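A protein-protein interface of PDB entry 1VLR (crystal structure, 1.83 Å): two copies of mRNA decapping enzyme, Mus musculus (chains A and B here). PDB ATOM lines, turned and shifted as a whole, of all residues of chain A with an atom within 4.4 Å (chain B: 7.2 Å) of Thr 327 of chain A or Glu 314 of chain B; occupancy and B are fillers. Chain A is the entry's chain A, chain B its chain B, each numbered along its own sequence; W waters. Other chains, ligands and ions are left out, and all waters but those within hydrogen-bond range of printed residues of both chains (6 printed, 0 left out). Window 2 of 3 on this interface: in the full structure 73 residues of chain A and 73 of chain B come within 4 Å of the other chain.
Of the 8 printed residues of chain A, 4 touch a printed residue of chain B. Printed residues of chain A that touch a printed residue of chain B: Arg 163, Arg 326, Thr 327 and Thr 329. Along chain A the printed residues that touch a printed residue of chain B span positions 163 to 329. Printed residues of chain B that touch a printed residue of chain A: Leu 308, Ala 310, Glu 314, Asn 315 and Cys 318. Among the printed residues, Asp or Glu carboxylates within 4 Å of a Lys or Arg side-chain nitrogen of the other chain: Arg 163 of chain A with Glu 314 of chain B (2.9 Å).
O of Gln 311 of chain B lies close to ND2 of Asn 315 of chain B (3.4 Å). The side-chain amide nitrogen of Asn 315 of chain B sits at hydrogen-bond distance from the side-chain hydroxyl of Tyr 323 of chain B (3.0 Å). The guanidinium group (NE) of Arg 163 of chain A is in hydrogen-bond range of the side-chain hydroxyl (OG1) of Thr 329 of chain A (2.8 Å). O of Glu 314 of chain B is in hydrogen-bond range of SG of Cys 318 of chain B (3.3 Å).
No position is printed for both chains. Of the 7 pairs that touch across the chains among the printed residues, none has its exchanged pair printed and touching as well.
Water W3 lies within hydrogen-bond range of O of Thr 327 of chain A, OE1 of Gln 311 of chain B, OG1 of Thr 329 of chain A and NH2 of Arg 163 of chain A. Water W6 lies within hydrogen-bond range of OE2 of Glu 314 of chain B and OG1 of Thr 327 of chain A. Water W2 lies within hydrogen-bond range of the side-chain carboxylate of Glu 314 of chain B (2.8 Å), the guanidinium group of Arg 326 of chain A (2.8 Å) and the backbone carbonyl oxygen of Thr 327 of chain A (2.9 Å). Water W4 lies within hydrogen-bond range of OE1 of Glu 314 of chain B, N of Thr 327 of chain A and NE of Arg 326 of chain A. Water W5 lies within hydrogen-bond range of the backbone NH (N) of Thr 329 of chain A (2.9 Å) and the side-chain amide oxygen (OE1) of Gln 311 of chain B (3.1 Å). Water W1 lies within hydrogen-bond range of ND1 of His 322 of chain B, O of Asn 315 of chain B and NH1 of Arg 326 of chain A.
Glu 164 of chain A touches none of the printed residues of chain B. Thr 165 of chain A touches none of the printed residues of chain B. Thr 327 of chain A touches just one residue of chain B: Glu 314. Of the printed residues of chain B, Thr 329 of chain A touches Leu 308 (3.7 Å). Of the printed residues of chain A, Ala 310 of chain B touches Arg 163. Glu 314 of chain B touches three residues of chain A. The nearest residue of chain B that does not touch Thr 327 of chain A is Gln 311 of chain B (4.4 Å). The nearest printed residue of chain A that does not touch Ala 310 of chain B is Thr 329 of chain A (5.4 Å).
The guanidinium group (NH2) of Arg 163 of chain A is in salt-bridge range of the side-chain carboxylate (OE1) of Glu 314 of chain B (2.9 Å). The guanidinium group (NH2) of Arg 326 of chain A lies within hydrogen-bond range of the side-chain amide oxygen (OD1) of Asn 315 of chain B (2.9 Å).
Among the printed residues, pairs that only touch across the chains: Arg 163 of chain A with Ala 310 of chain B (3.6 Å), Arg 326 of chain A with Glu 314 of chain B (3.6 Å), Arg 326 of chain A with Cys 318 of chain B (3.8 Å), Thr 327 of chain A with Glu 314 of chain B (3.5 Å) and Thr 329 of chain A with Leu 308 of chain B (3.7 Å).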
ATOM      1  N   ARG A 163     -12.843 -14.501 -23.164  1.00  0.00           N
ATOM      2  CA  ARG A 163     -13.501 -13.884 -22.027  1.00  0.00           C
ATOM      3  C   ARG A 163     -12.827 -12.521 -21.866  1.00  0.00           C
ATOM      4  O   ARG A 163     -11.710 -12.420 -21.325  1.00  0.00           O
ATOM      5  CB  ARG A 163     -13.377 -14.752 -20.816  1.00  0.00           C
ATOM      6  CG  ARG A 163     -13.980 -16.124 -21.037  1.00  0.00           C
ATOM      7  CD  ARG A 163     -14.493 -16.814 -19.798  1.00  0.00           C
ATOM      8  NE  ARG A 163     -15.550 -16.023 -19.131  1.00  0.00           N
ATOM      9  CZ  ARG A 163     -15.456 -15.448 -17.961  1.00  0.00           C
ATOM     10  NH1 ARG A 163     -14.333 -15.555 -17.199  1.00  0.00           N
ATOM     11  NH2 ARG A 163     -16.478 -14.751 -17.547  1.00  0.00           N
ATOM     12  N   GLU A 164     -13.525 -11.492 -22.353  1.00  0.00           N
ATOM     13  CA  GLU A 164     -12.971 -10.164 -22.448  1.00  0.00           C
ATOM     14  C   GLU A 164     -13.206  -9.395 -21.192  1.00  0.00           C
ATOM     15  O   GLU A 164     -14.379  -9.124 -20.819  1.00  0.00           O
ATOM     16  CB  GLU A 164     -13.638  -9.453 -23.640  1.00  0.00           C
ATOM     17  CG  GLU A 164     -13.214  -8.014 -23.850  1.00  0.00           C
ATOM     18  CD  GLU A 164     -14.222  -7.282 -24.745  1.00  0.00           C
ATOM     19  OE1 GLU A 164     -15.416  -7.209 -24.379  1.00  0.00           O
ATOM     20  OE2 GLU A 164     -13.831  -6.805 -25.811  1.00  0.00           O
ATOM     21  N   THR A 165     -12.160  -9.086 -20.448  1.00  0.00           N
ATOM     22  CA  THR A 165     -12.355  -8.294 -19.251  1.00  0.00           C
ATOM     23  C   THR A 165     -12.642  -6.841 -19.613  1.00  0.00           C
ATOM     24  O   THR A 165     -12.429  -6.419 -20.739  1.00  0.00           O
ATOM     25  CB  THR A 165     -11.098  -8.268 -18.325  1.00  0.00           C
ATOM     26  OG1 THR A 165     -10.036  -7.627 -19.024  1.00  0.00           O
ATOM     27  CG2 THR A 165     -10.643  -9.647 -17.953  1.00  0.00           C
ATOM     28  N   GLN A 325     -17.239  -2.989 -16.338  1.00  0.00           N
ATOM     29  CA  GLN A 325     -16.362  -3.674 -15.378  1.00  0.00           C
ATOM     30  C   GLN A 325     -16.344  -5.175 -15.551  1.00  0.00           C
ATOM     31  O   GLN A 325     -15.283  -5.793 -15.333  1.00  0.00           O
ATOM     32  CB  GLN A 325     -16.751  -3.338 -13.977  1.00  0.00           C
ATOM     33  CG  GLN A 325     -16.213  -1.920 -13.625  1.00  0.00           C
ATOM     34  CD  GLN A 325     -16.510  -1.494 -12.239  1.00  0.00           C
ATOM     35  OE1 GLN A 325     -17.280  -2.132 -11.549  1.00  0.00           O
ATOM     36  NE2 GLN A 325     -15.913  -0.362 -11.819  1.00  0.00           N
ATOM     37  N   ARG A 326     -17.478  -5.757 -15.930  1.00  0.00           N
ATOM     38  CA  ARG A 326     -17.585  -7.209 -16.005  1.00  0.00           C
ATOM     39  C   ARG A 326     -16.950  -7.794 -17.259  1.00  0.00           C
ATOM     40  O   ARG A 326     -16.866  -7.185 -18.315  1.00  0.00           O
ATOM     41  CB  ARG A 326     -19.041  -7.689 -15.914  1.00  0.00           C
ATOM     42  CG  ARG A 326     -19.699  -7.366 -14.601  1.00  0.00           C
ATOM     43  CD  ARG A 326     -19.140  -8.094 -13.382  1.00  0.00           C
ATOM     44  NE  ARG A 326     -19.255  -9.528 -13.609  1.00  0.00           N
ATOM     45  CZ  ARG A 326     -20.290 -10.277 -13.230  1.00  0.00           C
ATOM     46  NH1 ARG A 326     -21.289  -9.758 -12.538  1.00  0.00           N
ATOM     47  NH2 ARG A 326     -20.301 -11.541 -13.537  1.00  0.00           N
ATOM     48  N   THR A 327     -16.625  -9.088 -17.145  1.00  0.00           N
ATOM     49  CA  THR A 327     -16.093  -9.877 -18.210  1.00  0.00           C
ATOM     50  C   THR A 327     -17.219 -10.461 -19.045  1.00  0.00           C
ATOM     51  O   THR A 327     -18.149 -11.096 -18.500  1.00  0.00           O
ATOM     52  CB  THR A 327     -15.250 -10.965 -17.611  1.00  0.00           C
ATOM     53  OG1 THR A 327     -14.133 -10.347 -16.924  1.00  0.00           O
ATOM     54  CG2 THR A 327     -14.610 -11.880 -18.668  1.00  0.00           C
ATOM     55  N   LEU A 328     -17.134 -10.235 -20.338  1.00  0.00           N
ATOM     56  CA  LEU A 328     -18.134 -10.718 -21.291  1.00  0.00           C
ATOM     57  C   LEU A 328     -17.475 -11.796 -22.112  1.00  0.00           C
ATOM     58  O   LEU A 328     -16.295 -11.671 -22.523  1.00  0.00           O
ATOM     59  CB  LEU A 328     -18.590  -9.556 -22.190  1.00  0.00           C
ATOM     60  CG  LEU A 328     -19.281  -8.383 -21.501  1.00  0.00           C
ATOM     61  CD1 LEU A 328     -19.746  -7.407 -22.542  1.00  0.00           C
ATOM     62  CD2 LEU A 328     -20.433  -8.907 -20.744  1.00  0.00           C
ATOM     63  N   THR A 329     -18.233 -12.859 -22.369  1.00  0.00           N
ATOM     64  CA  THR A 329     -17.733 -14.004 -23.086  1.00  0.00           C
ATOM     65  C   THR A 329     -18.348 -14.110 -24.464  1.00  0.00           C
ATOM     66  O   THR A 329     -19.576 -14.077 -24.614  1.00  0.00           O
ATOM     67  CB  THR A 329     -18.090 -15.251 -22.292  1.00  0.00           C
ATOM     68  OG1 THR A 329     -17.517 -15.129 -20.986  1.00  0.00           O
ATOM     69  CG2 THR A 329     -17.517 -16.565 -22.953  1.00  0.00           C
ATOM     70  N   LEU B 249     -18.638 -22.170  -4.641  1.00  0.00           N
ATOM     71  CA  LEU B 249     -17.652 -21.665  -5.568  1.00  0.00           C
ATOM     72  C   LEU B 249     -16.516 -22.649  -5.816  1.00  0.00           C
ATOM     73  O   LEU B 249     -16.039 -22.822  -6.954  1.00  0.00           O
ATOM     74  CB  LEU B 249     -17.144 -20.263  -5.143  1.00  0.00           C
ATOM     75  CG  LEU B 249     -17.985 -19.074  -5.682  1.00  0.00           C
ATOM     76  CD1 LEU B 249     -17.724 -17.768  -4.918  1.00  0.00           C
ATOM     77  CD2 LEU B 249     -17.724 -18.877  -7.171  1.00  0.00           C
ATOM     78  N   LEU B 308     -23.390 -19.790 -18.621  1.00  0.00           N
ATOM     79  CA  LEU B 308     -21.982 -20.195 -18.721  1.00  0.00           C
ATOM     80  C   LEU B 308     -21.432 -20.344 -17.310  1.00  0.00           C
ATOM     81  O   LEU B 308     -21.584 -19.434 -16.501  1.00  0.00           O
ATOM     82  CB  LEU B 308     -21.173 -19.192 -19.491  1.00  0.00           C
ATOM     83  CG  LEU B 308     -21.479 -19.149 -20.986  1.00  0.00           C
ATOM     84  CD1 LEU B 308     -20.657 -18.014 -21.628  1.00  0.00           C
ATOM     85  CD2 LEU B 308     -21.212 -20.465 -21.678  1.00  0.00           C
ATOM     86  N   LEU B 309     -20.724 -21.428 -17.060  1.00  0.00           N
ATOM     87  CA  LEU B 309     -20.137 -21.680 -15.753  1.00  0.00           C
ATOM     88  C   LEU B 309     -19.203 -20.548 -15.295  1.00  0.00           C
ATOM     89  O   LEU B 309     -19.218 -20.134 -14.109  1.00  0.00           O
ATOM     90  CB  LEU B 309     -19.399 -23.031 -15.764  1.00  0.00           C
ATOM     91  CG  LEU B 309     -18.723 -23.461 -14.446  1.00  0.00           C
ATOM     92  CD1 LEU B 309     -19.620 -23.376 -13.193  1.00  0.00           C
ATOM     93  CD2 LEU B 309     -18.224 -24.895 -14.663  1.00  0.00           C
ATOM     94  N   ALA B 310     -18.368 -20.078 -16.209  1.00  0.00           N
ATOM     95  CA  ALA B 310     -17.431 -18.997 -15.850  1.00  0.00           C
ATOM     96  C   ALA B 310     -18.159 -17.788 -15.370  1.00  0.00           C
ATOM     97  O   ALA B 310     -17.745 -17.155 -14.442  1.00  0.00           O
ATOM     98  CB  ALA B 310     -16.595 -18.684 -16.999  1.00  0.00           C
ATOM     99  N   GLN B 311     -19.302 -17.493 -15.998  1.00  0.00           N
ATOM    100  CA  GLN B 311     -20.091 -16.344 -15.632  1.00  0.00           C
ATOM    101  C   GLN B 311     -20.857 -16.561 -14.334  1.00  0.00           C
ATOM    102  O   GLN B 311     -20.999 -15.651 -13.535  1.00  0.00           O
ATOM    103  CB  GLN B 311     -21.046 -16.020 -16.785  1.00  0.00           C
ATOM    104  CG  GLN B 311     -21.792 -14.678 -16.592  1.00  0.00           C
ATOM    105  CD  GLN B 311     -22.249 -14.139 -17.897  1.00  0.00           C
ATOM    106  OE1 GLN B 311     -21.442 -13.944 -18.799  1.00  0.00           O
ATOM    107  NE2 GLN B 311     -23.584 -13.946 -18.038  1.00  0.00           N
ATOM    108  N   VAL B 312     -21.354 -17.783 -14.117  1.00  0.00           N
ATOM    109  CA  VAL B 312     -21.961 -18.166 -12.831  1.00  0.00           C
ATOM    110  C   VAL B 312     -20.997 -17.917 -11.693  1.00  0.00           C
ATOM    111  O   VAL B 312     -21.366 -17.336 -10.700  1.00  0.00           O
ATOM    112  CB  VAL B 312     -22.437 -19.661 -12.832  1.00  0.00           C
ATOM    113  CG1 VAL B 312     -22.885 -20.108 -11.492  1.00  0.00           C
ATOM    114  CG2 VAL B 312     -23.622 -19.819 -13.840  1.00  0.00           C
ATOM    115  N   ILE B 313     -19.760 -18.361 -11.858  1.00  0.00           N
ATOM    116  CA  ILE B 313     -18.753 -18.168 -10.842  1.00  0.00           C
ATOM    117  C   ILE B 313     -18.559 -16.681 -10.603  1.00  0.00           C
ATOM    118  O   ILE B 313     -18.540 -16.220  -9.457  1.00  0.00           O
ATOM    119  CB  ILE B 313     -17.440 -18.849 -11.293  1.00  0.00           C
ATOM    120  CG1 ILE B 313     -17.595 -20.393 -11.225  1.00  0.00           C
ATOM    121  CG2 ILE B 313     -16.169 -18.329 -10.508  1.00  0.00           C
ATOM    122  CD1 ILE B 313     -16.486 -21.107 -12.001  1.00  0.00           C
ATOM    123  N   GLU B 314     -18.445 -15.900 -11.665  1.00  0.00           N
ATOM    124  CA  GLU B 314     -18.159 -14.480 -11.475  1.00  0.00           C
ATOM    125  C   GLU B 314     -19.332 -13.747 -10.860  1.00  0.00           C
ATOM    126  O   GLU B 314     -19.150 -12.826 -10.037  1.00  0.00           O
ATOM    127  CB  GLU B 314     -17.704 -13.868 -12.753  1.00  0.00           C
ATOM    128  CG  GLU B 314     -16.259 -14.260 -13.018  1.00  0.00           C
ATOM    129  CD  GLU B 314     -15.714 -13.804 -14.343  1.00  0.00           C
ATOM    130  OE1 GLU B 314     -16.435 -13.119 -15.130  1.00  0.00           O
ATOM    131  OE2 GLU B 314     -14.531 -14.169 -14.635  1.00  0.00           O
ATOM    132  N   ASN B 315     -20.530 -14.159 -11.256  1.00  0.00           N
ATOM    133  CA  ASN B 315     -21.756 -13.664 -10.639  1.00  0.00           C
ATOM    134  C   ASN B 315     -21.730 -13.828  -9.131  1.00  0.00           C
ATOM    135  O   ASN B 315     -22.033 -12.892  -8.405  1.00  0.00           O
ATOM    136  CB  ASN B 315     -22.998 -14.309 -11.219  1.00  0.00           C
ATOM    137  CG  ASN B 315     -23.363 -13.760 -12.588  1.00  0.00           C
ATOM    138  OD1 ASN B 315     -22.864 -12.688 -13.011  1.00  0.00           O
ATOM    139  ND2 ASN B 315     -24.230 -14.490 -13.310  1.00  0.00           N
ATOM    140  N   LEU B 316     -21.418 -15.036  -8.676  1.00  0.00           N
ATOM    141  CA  LEU B 316     -21.304 -15.335  -7.274  1.00  0.00           C
ATOM    142  C   LEU B 316     -20.199 -14.566  -6.598  1.00  0.00           C
ATOM    143  O   LEU B 316     -20.328 -14.198  -5.409  1.00  0.00           O
ATOM    144  CB  LEU B 316     -21.075 -16.811  -7.032  1.00  0.00           C
ATOM    145  CG  LEU B 316     -22.273 -17.722  -7.279  1.00  0.00           C
ATOM    146  CD1 LEU B 316     -21.855 -19.190  -7.406  1.00  0.00           C
ATOM    147  CD2 LEU B 316     -23.217 -17.507  -6.103  1.00  0.00           C
ATOM    148  N   GLU B 317     -19.117 -14.328  -7.319  1.00  0.00           N
ATOM    149  CA  GLU B 317     -17.986 -13.576  -6.724  1.00  0.00           C
ATOM    150  C   GLU B 317     -18.396 -12.138  -6.523  1.00  0.00           C
ATOM    151  O   GLU B 317     -17.973 -11.490  -5.544  1.00  0.00           O
ATOM    152  CB  GLU B 317     -16.778 -13.678  -7.632  1.00  0.00           C
ATOM    153  CG  GLU B 317     -16.160 -15.043  -7.527  1.00  0.00           C
ATOM    154  CD  GLU B 317     -15.045 -15.308  -8.503  1.00  0.00           C
ATOM    155  OE1 GLU B 317     -14.932 -14.574  -9.496  1.00  0.00           O
ATOM    156  OE2 GLU B 317     -14.253 -16.275  -8.257  1.00  0.00           O
ATOM    157  N   CYS B 318     -19.198 -11.633  -7.450  1.00  0.00           N
ATOM    158  CA  CYS B 318     -19.597 -10.215  -7.441  1.00  0.00           C
ATOM    159  C   CYS B 318     -20.717  -9.965  -6.464  1.00  0.00           C
ATOM    160  O   CYS B 318     -20.742  -8.914  -5.819  1.00  0.00           O
ATOM    161  CB  CYS B 318     -19.980  -9.720  -8.836  1.00  0.00           C
ATOM    162  SG  CYS B 318     -18.539  -9.545  -9.868  1.00  0.00           S
ATOM    163  N   ASP B 319     -21.672 -10.891  -6.384  1.00  0.00           N
ATOM    164  CA  ASP B 319     -22.791 -10.777  -5.486  1.00  0.00           C
ATOM    165  C   ASP B 319     -23.131 -12.108  -4.938  1.00  0.00           C
ATOM    166  O   ASP B 319     -23.693 -12.939  -5.662  1.00  0.00           O
ATOM    167  CB  ASP B 319     -24.079 -10.279  -6.111  1.00  0.00           C
ATOM    168  CG  ASP B 319     -25.188 -10.022  -5.011  1.00  0.00           C
ATOM    169  OD1 ASP B 319     -25.210 -10.534  -3.804  1.00  0.00           O
ATOM    170  OD2 ASP B 319     -26.133  -9.249  -5.270  1.00  0.00           O
ATOM    171  N   HIS B 322     -26.671 -13.526  -5.517  1.00  0.00           N
ATOM    172  CA  HIS B 322     -27.165 -13.354  -6.871  1.00  0.00           C
ATOM    173  C   HIS B 322     -28.251 -14.340  -7.206  1.00  0.00           C
ATOM    174  O   HIS B 322     -29.304 -13.944  -7.679  1.00  0.00           O
ATOM    175  CB  HIS B 322     -26.002 -13.639  -7.832  1.00  0.00           C
ATOM    176  CG  HIS B 322     -26.330 -13.417  -9.254  1.00  0.00           C
ATOM    177  ND1 HIS B 322     -26.107 -12.209  -9.882  1.00  0.00           N
ATOM    178  CD2 HIS B 322     -26.903 -14.229 -10.181  1.00  0.00           C
ATOM    179  CE1 HIS B 322     -26.492 -12.295 -11.142  1.00  0.00           C
ATOM    180  NE2 HIS B 322     -26.976 -13.515 -11.351  1.00  0.00           N
ATOM    181  N   TYR B 323     -28.007 -15.627  -6.940  1.00  0.00           N
ATOM    182  CA  TYR B 323     -28.924 -16.647  -7.421  1.00  0.00           C
ATOM    183  C   TYR B 323     -30.175 -16.823  -6.584  1.00  0.00           C
ATOM    184  O   TYR B 323     -31.108 -17.486  -7.018  1.00  0.00           O
ATOM    185  CB  TYR B 323     -28.225 -18.008  -7.707  1.00  0.00           C
ATOM    186  CG  TYR B 323     -27.399 -17.857  -8.932  1.00  0.00           C
ATOM    187  CD1 TYR B 323     -27.985 -17.849 -10.190  1.00  0.00           C
ATOM    188  CD2 TYR B 323     -26.038 -17.619  -8.863  1.00  0.00           C
ATOM    189  CE1 TYR B 323     -27.261 -17.644 -11.328  1.00  0.00           C
ATOM    190  CE2 TYR B 323     -25.292 -17.413 -10.012  1.00  0.00           C
ATOM    191  CZ  TYR B 323     -25.905 -17.378 -11.246  1.00  0.00           C
ATOM    192  OH  TYR B 323     -25.214 -17.125 -12.394  1.00  0.00           O
HETATM  193  O   HOH W   1     -23.456 -10.495 -10.059  1.00  0.00           O
HETATM  194  O   HOH W   2     -18.896 -12.131 -15.865  1.00  0.00           O
HETATM  195  O   HOH W   3     -18.721 -13.552 -19.051  1.00  0.00           O
HETATM  196  O   HOH W   4     -16.628 -10.363 -14.550  1.00  0.00           O
HETATM  197  O   HOH W   5     -21.048 -12.659 -21.538  1.00  0.00           O
HETATM  198  O   HOH W   6     -12.866 -12.330 -15.556  1.00  0.00           O
